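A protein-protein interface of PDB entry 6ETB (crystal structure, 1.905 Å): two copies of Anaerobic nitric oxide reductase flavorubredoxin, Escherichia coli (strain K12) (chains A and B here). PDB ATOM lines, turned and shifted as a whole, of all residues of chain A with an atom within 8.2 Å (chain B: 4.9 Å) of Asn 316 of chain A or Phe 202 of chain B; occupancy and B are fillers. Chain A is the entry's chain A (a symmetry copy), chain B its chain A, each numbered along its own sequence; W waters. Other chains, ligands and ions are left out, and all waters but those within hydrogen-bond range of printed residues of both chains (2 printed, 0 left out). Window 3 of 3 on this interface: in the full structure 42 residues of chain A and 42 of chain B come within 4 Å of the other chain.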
ATOM      1  N   MET A 261     -15.541   0.850  32.325  1.00  0.00           N
ATOM      2  CA  MET A 261     -16.314   1.487  31.263  1.00  0.00           C
ATOM      3  C   MET A 261     -17.789   1.092  31.304  1.00  0.00           C
ATOM      4  O   MET A 261     -18.655   1.868  30.903  1.00  0.00           O
ATOM      5  CB  MET A 261     -15.717   1.145  29.896  1.00  0.00           C
ATOM      6  CG  MET A 261     -14.309   1.687  29.687  1.00  0.00           C
ATOM      7  SD  MET A 261     -13.627   1.308  28.061  1.00  0.00           S
ATOM      8  CE  MET A 261     -13.462  -0.473  28.166  1.00  0.00           C
ATOM      9  N   SER A 313     -10.120  -2.830  32.725  1.00  0.00           N
ATOM     10  CA  SER A 313     -10.619  -3.575  31.582  1.00  0.00           C
ATOM     11  C   SER A 313      -9.625  -3.462  30.439  1.00  0.00           C
ATOM     12  O   SER A 313      -8.743  -2.603  30.461  1.00  0.00           O
ATOM     13  CB  SER A 313     -11.991  -3.060  31.152  1.00  0.00           C
ATOM     14  OG  SER A 313     -11.959  -1.669  30.895  1.00  0.00           O
ATOM     15  N   THR A 314      -9.759  -4.329  29.443  1.00  0.00           N
ATOM     16  CA  THR A 314      -8.878  -4.256  28.288  1.00  0.00           C
ATOM     17  C   THR A 314      -9.432  -3.255  27.286  1.00  0.00           C
ATOM     18  O   THR A 314     -10.557  -3.394  26.805  1.00  0.00           O
ATOM     19  CB  THR A 314      -8.693  -5.624  27.611  1.00  0.00           C
ATOM     20  OG1 THR A 314      -8.167  -6.560  28.558  1.00  0.00           O
ATOM     21  CG2 THR A 314      -7.725  -5.505  26.448  1.00  0.00           C
ATOM     22  N   MET A 315      -8.637  -2.234  26.994  1.00  0.00           N
ATOM     23  CA  MET A 315      -9.034  -1.182  26.068  1.00  0.00           C
ATOM     24  C   MET A 315      -7.990  -1.044  24.970  1.00  0.00           C
ATOM     25  O   MET A 315      -6.881  -0.576  25.224  1.00  0.00           O
ATOM     26  CB  MET A 315      -9.213   0.142  26.816  1.00  0.00           C
ATOM     27  CG  MET A 315      -9.477   1.349  25.931  1.00  0.00           C
ATOM     28  SD  MET A 315      -9.499   2.886  26.882  1.00  0.00           S
ATOM     29  CE  MET A 315      -9.706   4.091  25.574  1.00  0.00           C
ATOM     30  N   ASN A 316      -8.347  -1.457  23.757  1.00  0.00           N
ATOM     31  CA  ASN A 316      -7.420  -1.458  22.626  1.00  0.00           C
ATOM     32  C   ASN A 316      -6.143  -2.231  22.954  1.00  0.00           C
ATOM     33  O   ASN A 316      -5.036  -1.752  22.704  1.00  0.00           O
ATOM     34  CB  ASN A 316      -7.081  -0.025  22.200  1.00  0.00           C
ATOM     35  CG  ASN A 316      -8.299   0.745  21.721  1.00  0.00           C
ATOM     36  OD1 ASN A 316      -9.183   0.187  21.071  1.00  0.00           O
ATOM     37  ND2 ASN A 316      -8.352   2.032  22.047  1.00  0.00           N
ATOM     38  N   ASN A 317      -6.324  -3.414  23.540  1.00  0.00           N
ATOM     39  CA  ASN A 317      -5.238  -4.330  23.901  1.00  0.00           C
ATOM     40  C   ASN A 317      -4.303  -3.818  25.001  1.00  0.00           C
ATOM     41  O   ASN A 317      -3.320  -4.479  25.336  1.00  0.00           O
ATOM     42  CB  ASN A 317      -4.412  -4.685  22.662  1.00  0.00           C
ATOM     43  CG  ASN A 317      -5.264  -5.224  21.531  1.00  0.00           C
ATOM     44  OD1 ASN A 317      -5.744  -6.355  21.583  1.00  0.00           O
ATOM     45  ND2 ASN A 317      -5.462  -4.409  20.499  1.00  0.00           N
ATOM     46  N   VAL A 318      -4.603  -2.652  25.563  1.00  0.00           N
ATOM     47  CA  VAL A 318      -3.837  -2.143  26.698  1.00  0.00           C
ATOM     48  C   VAL A 318      -4.768  -1.817  27.861  1.00  0.00           C
ATOM     49  O   VAL A 318      -5.977  -2.041  27.777  1.00  0.00           O
ATOM     50  CB  VAL A 318      -3.014  -0.889  26.330  1.00  0.00           C
ATOM     51  CG1 VAL A 318      -2.025  -1.208  25.215  1.00  0.00           C
ATOM     52  CG2 VAL A 318      -3.926   0.260  25.932  1.00  0.00           C
ATOM     53  N   MET A 319      -4.206  -1.298  28.946  1.00  0.00           N
ATOM     54  CA  MET A 319      -5.002  -0.989  30.128  1.00  0.00           C
ATOM     55  C   MET A 319      -5.545   0.433  30.054  1.00  0.00           C
ATOM     56  O   MET A 319      -5.103   1.235  29.231  1.00  0.00           O
ATOM     57  CB  MET A 319      -4.174  -1.175  31.404  1.00  0.00           C
ATOM     58  CG  MET A 319      -3.165  -0.070  31.668  1.00  0.00           C
ATOM     59  SD  MET A 319      -2.073  -0.445  33.057  1.00  0.00           S
ATOM     60  CE  MET A 319      -1.075  -1.751  32.354  1.00  0.00           C
ATOM     61  N   MET A 320      -6.507   0.742  30.916  1.00  0.00           N
ATOM     62  CA  MET A 320      -7.089   2.076  30.948  1.00  0.00           C
ATOM     63  C   MET A 320      -6.059   3.081  31.462  1.00  0.00           C
ATOM     64  O   MET A 320      -5.390   2.830  32.464  1.00  0.00           O
ATOM     65  CB  MET A 320      -8.354   2.086  31.807  1.00  0.00           C
ATOM     66  CG  MET A 320      -9.419   1.119  31.302  1.00  0.00           C
ATOM     67  SD  MET A 320     -11.037   1.328  32.066  1.00  0.00           S
ATOM     68  CE  MET A 320     -11.431   3.000  31.558  1.00  0.00           C
ATOM     69  N   TRP A 348     -12.707 -10.113  24.527  1.00  0.00           N
ATOM     70  CA  TRP A 348     -12.282 -11.268  23.743  1.00  0.00           C
ATOM     71  C   TRP A 348     -10.892 -11.773  24.131  1.00  0.00           C
ATOM     72  O   TRP A 348     -10.770 -12.713  24.915  1.00  0.00           O
ATOM     73  CB  TRP A 348     -12.333 -10.943  22.243  1.00  0.00           C
ATOM     74  CG  TRP A 348     -11.879  -9.558  21.864  1.00  0.00           C
ATOM     75  CD1 TRP A 348     -10.657  -9.200  21.373  1.00  0.00           C
ATOM     76  CD2 TRP A 348     -12.652  -8.351  21.927  1.00  0.00           C
ATOM     77  NE1 TRP A 348     -10.619  -7.848  21.134  1.00  0.00           N
ATOM     78  CE2 TRP A 348     -11.831  -7.303  21.466  1.00  0.00           C
ATOM     79  CE3 TRP A 348     -13.958  -8.055  22.331  1.00  0.00           C
ATOM     80  CZ2 TRP A 348     -12.272  -5.984  21.397  1.00  0.00           C
ATOM     81  CZ3 TRP A 348     -14.392  -6.743  22.267  1.00  0.00           C
ATOM     82  CH2 TRP A 348     -13.552  -5.724  21.802  1.00  0.00           C
ATOM     83  N   SER A 349      -9.849 -11.153  23.586  1.00  0.00           N
ATOM     84  CA  SER A 349      -8.486 -11.629  23.804  1.00  0.00           C
ATOM     85  C   SER A 349      -7.866 -11.081  25.089  1.00  0.00           C
ATOM     86  O   SER A 349      -6.945 -11.682  25.644  1.00  0.00           O
ATOM     87  CB  SER A 349      -7.602 -11.270  22.606  1.00  0.00           C
ATOM     88  OG  SER A 349      -7.679  -9.888  22.305  1.00  0.00           O
ATOM     89  N   GLY A 350      -8.371  -9.944  25.557  1.00  0.00           N
ATOM     90  CA  GLY A 350      -7.874  -9.328  26.777  1.00  0.00           C
ATOM     91  C   GLY A 350      -6.399  -8.979  26.711  1.00  0.00           C
ATOM     92  O   GLY A 350      -5.887  -8.614  25.653  1.00  0.00           O
ATOM     93  N   ALA A 352      -4.858  -6.860  29.179  1.00  0.00           N
ATOM     94  CA  ALA A 352      -4.586  -5.707  30.031  1.00  0.00           C
ATOM     95  C   ALA A 352      -4.281  -6.118  31.468  1.00  0.00           C
ATOM     96  O   ALA A 352      -3.467  -5.485  32.140  1.00  0.00           O
ATOM     97  CB  ALA A 352      -5.754  -4.741  30.000  1.00  0.00           C
ATOM     98  N   ARG A 355      -0.810  -7.364  31.622  1.00  0.00           N
ATOM     99  CA  ARG A 355      -0.001  -6.167  31.425  1.00  0.00           C
ATOM    100  C   ARG A 355       0.089  -5.347  32.709  1.00  0.00           C
ATOM    101  O   ARG A 355       1.146  -4.815  33.050  1.00  0.00           O
ATOM    102  CB  ARG A 355      -0.588  -5.325  30.289  1.00  0.00           C
ATOM    103  CG  ARG A 355       0.229  -4.106  29.897  1.00  0.00           C
ATOM    104  CD  ARG A 355      -0.458  -3.349  28.767  1.00  0.00           C
ATOM    105  NE  ARG A 355       0.194  -2.079  28.464  1.00  0.00           N
ATOM    106  CZ  ARG A 355       1.175  -1.933  27.579  1.00  0.00           C
ATOM    107  NH1 ARG A 355       1.627  -2.982  26.906  1.00  0.00           N
ATOM    108  NH2 ARG A 355       1.706  -0.737  27.368  1.00  0.00           N
ATOM    109  N   MET B 145     -14.211  -6.791  14.195  1.00  0.00           N
ATOM    110  CA  MET B 145     -13.229  -5.821  14.678  1.00  0.00           C
ATOM    111  C   MET B 145     -13.388  -4.446  14.035  1.00  0.00           C
ATOM    112  O   MET B 145     -12.424  -3.689  13.920  1.00  0.00           O
ATOM    113  CB  MET B 145     -11.807  -6.343  14.464  1.00  0.00           C
ATOM    114  CG  MET B 145     -11.472  -7.545  15.324  1.00  0.00           C
ATOM    115  SD  MET B 145     -11.921  -7.276  17.050  1.00  0.00           S
ATOM    116  CE  MET B 145     -10.851  -5.907  17.480  1.00  0.00           C
ATOM    117  N   LEU B 146     -14.611  -4.127  13.621  1.00  0.00           N
ATOM    118  CA  LEU B 146     -14.940  -2.777  13.170  1.00  0.00           C
ATOM    119  C   LEU B 146     -16.213  -2.265  13.845  1.00  0.00           C
ATOM    120  O   LEU B 146     -17.270  -2.203  13.217  1.00  0.00           O
ATOM    121  CB  LEU B 146     -15.101  -2.738  11.649  1.00  0.00           C
ATOM    122  CG  LEU B 146     -13.834  -2.941  10.815  1.00  0.00           C
ATOM    123  CD1 LEU B 146     -14.170  -2.988   9.332  1.00  0.00           C
ATOM    124  CD2 LEU B 146     -12.823  -1.839  11.101  1.00  0.00           C
ATOM    125  N   HIS B 147     -16.115  -1.896  15.122  1.00  0.00           N
ATOM    126  CA  HIS B 147     -14.855  -1.948  15.858  1.00  0.00           C
ATOM    127  C   HIS B 147     -14.875  -3.025  16.946  1.00  0.00           C
ATOM    128  O   HIS B 147     -13.997  -3.064  17.808  1.00  0.00           O
ATOM    129  CB  HIS B 147     -14.530  -0.580  16.461  1.00  0.00           C
ATOM    130  CG  HIS B 147     -15.619  -0.018  17.318  1.00  0.00           C
ATOM    131  ND1 HIS B 147     -15.606  -0.111  18.693  1.00  0.00           N
ATOM    132  CD2 HIS B 147     -16.754   0.648  16.997  1.00  0.00           C
ATOM    133  CE1 HIS B 147     -16.685   0.476  19.182  1.00  0.00           C
ATOM    134  NE2 HIS B 147     -17.399   0.941  18.174  1.00  0.00           N
ATOM    135  N   ILE B 198     -11.469   6.298  18.395  1.00  0.00           N
ATOM    136  CA  ILE B 198     -12.087   4.979  18.490  1.00  0.00           C
ATOM    137  C   ILE B 198     -11.622   4.008  17.407  1.00  0.00           C
ATOM    138  O   ILE B 198     -11.314   2.852  17.694  1.00  0.00           O
ATOM    139  CB  ILE B 198     -13.629   5.080  18.422  1.00  0.00           C
ATOM    140  CG1 ILE B 198     -14.151   6.088  19.449  1.00  0.00           C
ATOM    141  CG2 ILE B 198     -14.270   3.714  18.628  1.00  0.00           C
ATOM    142  CD1 ILE B 198     -13.813   5.736  20.880  1.00  0.00           C
ATOM    143  N   LEU B 199     -11.560   4.480  16.165  1.00  0.00           N
ATOM    144  CA  LEU B 199     -11.370   3.589  15.025  1.00  0.00           C
ATOM    145  C   LEU B 199      -9.945   3.549  14.471  1.00  0.00           C
ATOM    146  O   LEU B 199      -9.663   2.792  13.543  1.00  0.00           O
ATOM    147  CB  LEU B 199     -12.335   3.983  13.906  1.00  0.00           C
ATOM    148  CG  LEU B 199     -13.805   4.056  14.324  1.00  0.00           C
ATOM    149  CD1 LEU B 199     -14.692   4.350  13.130  1.00  0.00           C
ATOM    150  CD2 LEU B 199     -14.230   2.763  14.997  1.00  0.00           C
ATOM    151  N   THR B 200      -9.053   4.354  15.040  1.00  0.00           N
ATOM    152  CA  THR B 200      -7.666   4.406  14.574  1.00  0.00           C
ATOM    153  C   THR B 200      -6.947   3.041  14.562  1.00  0.00           C
ATOM    154  O   THR B 200      -6.328   2.691  13.556  1.00  0.00           O
ATOM    155  CB  THR B 200      -6.831   5.401  15.414  1.00  0.00           C
ATOM    156  OG1 THR B 200      -7.401   6.710  15.313  1.00  0.00           O
ATOM    157  CG2 THR B 200      -5.391   5.444  14.922  1.00  0.00           C
ATOM    158  N   PRO B 201      -7.030   2.257  15.658  1.00  0.00           N
ATOM    159  CA  PRO B 201      -6.275   0.997  15.622  1.00  0.00           C
ATOM    160  C   PRO B 201      -6.836  -0.060  14.666  1.00  0.00           C
ATOM    161  O   PRO B 201      -6.172  -1.071  14.434  1.00  0.00           O
ATOM    162  CB  PRO B 201      -6.358   0.502  17.068  1.00  0.00           C
ATOM    163  CG  PRO B 201      -7.617   1.085  17.587  1.00  0.00           C
ATOM    164  CD  PRO B 201      -7.711   2.440  16.956  1.00  0.00           C
ATOM    165  N   PHE B 202      -8.028   0.164  14.123  1.00  0.00           N
ATOM    166  CA  PHE B 202      -8.638  -0.801  13.212  1.00  0.00           C
ATOM    167  C   PHE B 202      -8.586  -0.317  11.766  1.00  0.00           C
ATOM    168  O   PHE B 202      -9.332  -0.799  10.913  1.00  0.00           O
ATOM    169  CB  PHE B 202     -10.088  -1.082  13.616  1.00  0.00           C
ATOM    170  CG  PHE B 202     -10.285  -1.237  15.096  1.00  0.00           C
ATOM    171  CD1 PHE B 202      -9.801  -2.352  15.761  1.00  0.00           C
ATOM    172  CD2 PHE B 202     -10.963  -0.273  15.822  1.00  0.00           C
ATOM    173  CE1 PHE B 202      -9.981  -2.496  17.124  1.00  0.00           C
ATOM    174  CE2 PHE B 202     -11.148  -0.412  17.186  1.00  0.00           C
ATOM    175  CZ  PHE B 202     -10.656  -1.526  17.837  1.00  0.00           C
ATOM    176  N   SER B 203      -7.692   0.630  11.498  1.00  0.00           N
ATOM    177  CA  SER B 203      -7.603   1.263  10.186  1.00  0.00           C
ATOM    178  C   SER B 203      -7.212   0.283   9.082  1.00  0.00           C
ATOM    179  O   SER B 203      -7.637   0.430   7.938  1.00  0.00           O
ATOM    180  CB  SER B 203      -6.604   2.420  10.228  1.00  0.00           C
ATOM    181  OG  SER B 203      -7.059   3.452  11.085  1.00  0.00           O
ATOM    182  N   ARG B 204      -6.407  -0.716   9.429  1.00  0.00           N
ATOM    183  CA  ARG B 204      -5.960  -1.711   8.458  1.00  0.00           C
ATOM    184  C   ARG B 204      -7.114  -2.550   7.918  1.00  0.00           C
ATOM    185  O   ARG B 204      -7.008  -3.148   6.848  1.00  0.00           O
ATOM    186  CB  ARG B 204      -4.905  -2.627   9.082  1.00  0.00           C
ATOM    187  CG  ARG B 204      -3.534  -1.992   9.221  1.00  0.00           C
ATOM    188  CD  ARG B 204      -2.924  -1.719   7.857  1.00  0.00           C
ATOM    189  NE  ARG B 204      -2.784  -2.943   7.073  1.00  0.00           N
ATOM    190  CZ  ARG B 204      -1.720  -3.739   7.118  1.00  0.00           C
ATOM    191  NH1 ARG B 204      -0.698  -3.440   7.909  1.00  0.00           N
ATOM    192  NH2 ARG B 204      -1.677  -4.835   6.371  1.00  0.00           N
ATOM    193  N   LEU B 205      -8.215  -2.589   8.661  1.00  0.00           N
ATOM    194  CA  LEU B 205      -9.368  -3.403   8.289  1.00  0.00           C
ATOM    195  C   LEU B 205     -10.432  -2.598   7.545  1.00  0.00           C
ATOM    196  O   LEU B 205     -11.338  -3.170   6.938  1.00  0.00           O
ATOM    197  CB  LEU B 205      -9.981  -4.044   9.534  1.00  0.00           C
ATOM    198  CG  LEU B 205      -9.021  -4.858  10.403  1.00  0.00           C
ATOM    199  CD1 LEU B 205      -9.692  -5.255  11.707  1.00  0.00           C
ATOM    200  CD2 LEU B 205      -8.527  -6.087   9.651  1.00  0.00           C
ATOM    201  N   VAL B 206     -10.321  -1.275   7.600  1.00  0.00           N
ATOM    202  CA  VAL B 206     -11.330  -0.394   7.018  1.00  0.00           C
ATOM    203  C   VAL B 206     -11.395  -0.500   5.494  1.00  0.00           C
ATOM    204  O   VAL B 206     -12.454  -0.777   4.931  1.00  0.00           O
ATOM    205  CB  VAL B 206     -11.077   1.079   7.408  1.00  0.00           C
ATOM    206  CG1 VAL B 206     -12.026   2.001   6.659  1.00  0.00           C
ATOM    207  CG2 VAL B 206     -11.221   1.263   8.913  1.00  0.00           C
ATOM    208  N   GLY B 332      -2.295   1.820  22.407  1.00  0.00           N
ATOM    209  CA  GLY B 332      -3.453   1.041  22.010  1.00  0.00           C
ATOM    210  C   GLY B 332      -4.051   1.502  20.693  1.00  0.00           C
ATOM    211  O   GLY B 332      -4.547   0.691  19.911  1.00  0.00           O
ATOM    212  N   LEU B 333      -4.003   2.808  20.447  1.00  0.00           N
ATOM    213  CA  LEU B 333      -4.565   3.379  19.228  1.00  0.00           C
ATOM    214  C   LEU B 333      -3.711   3.061  18.003  1.00  0.00           C
ATOM    215  O   LEU B 333      -4.206   3.080  16.877  1.00  0.00           O
ATOM    216  CB  LEU B 333      -4.728   4.893  19.371  1.00  0.00           C
ATOM    217  CG  LEU B 333      -5.801   5.349  20.362  1.00  0.00           C
ATOM    218  CD1 LEU B 333      -5.853   6.869  20.444  1.00  0.00           C
ATOM    219  CD2 LEU B 333      -7.160   4.774  19.982  1.00  0.00           C
HETATM  220  O   HOH W   1     -11.360   1.805  20.246  1.00  0.00           O
HETATM  221  O   HOH W   2      -4.353  -1.877  19.433  1.00  0.00           O
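CG of Pro 201 of chain B touches OD1 of Asn 316 of chain A, 3.9 Å away. Phe 202 of chain B touches Asn 316 of chain A. Gly 332 of chain B touches Asn 316 of chain A (CA to O, 3.3 Å). Asn 316 of chain A touches Leu 333 of chain B.
Of chain B, only Pro 201, Phe 202, Gly 332 and Leu 333 come within 4 Å of Asn 316 of chain A. Met 319 of chain A touches none of the printed residues of chain B. Ser 349 of chain A touches none of the printed residues of chain B. Of the printed residues of chain A, Phe 202 of chain B touches Asn 316 (3.9 Å). No residue of chain A comes within 4 Å of Ser 203 of chain B. Printed residues of chain A within 4 Å of Gly 332 of chain B: Asn 316. Of the printed residues of chain A, Leu 333 of chain B touches Asn 316.
Of the 14 printed residues of chain B, 4 touch a printed residue of chain A. Hydrophobic or aromatic side chains of chain B that line the printed part of chain A: Pro 201, Phe 202 and Leu 333. Of the 14 printed residues of chain A, 1 touches a printed residue of chain B.
No position is printed for both chains. Of the 4 pairs that touch across the chains among the printed residues, none has its exchanged pair printed and touching as well.
Water W2 lies within hydrogen-bond range of the backbone carbonyl oxygen (O) of Gly 332 of chain B, the side-chain amide nitrogen (ND2) of Asn 317 of chain A and the backbone carbonyl oxygen (O) of Asn 316 of chain A. Water W1 bridges O of Ile 198 of chain B (2.8 Å) and OD1 of Asn 316 of chain A (2.8 Å).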
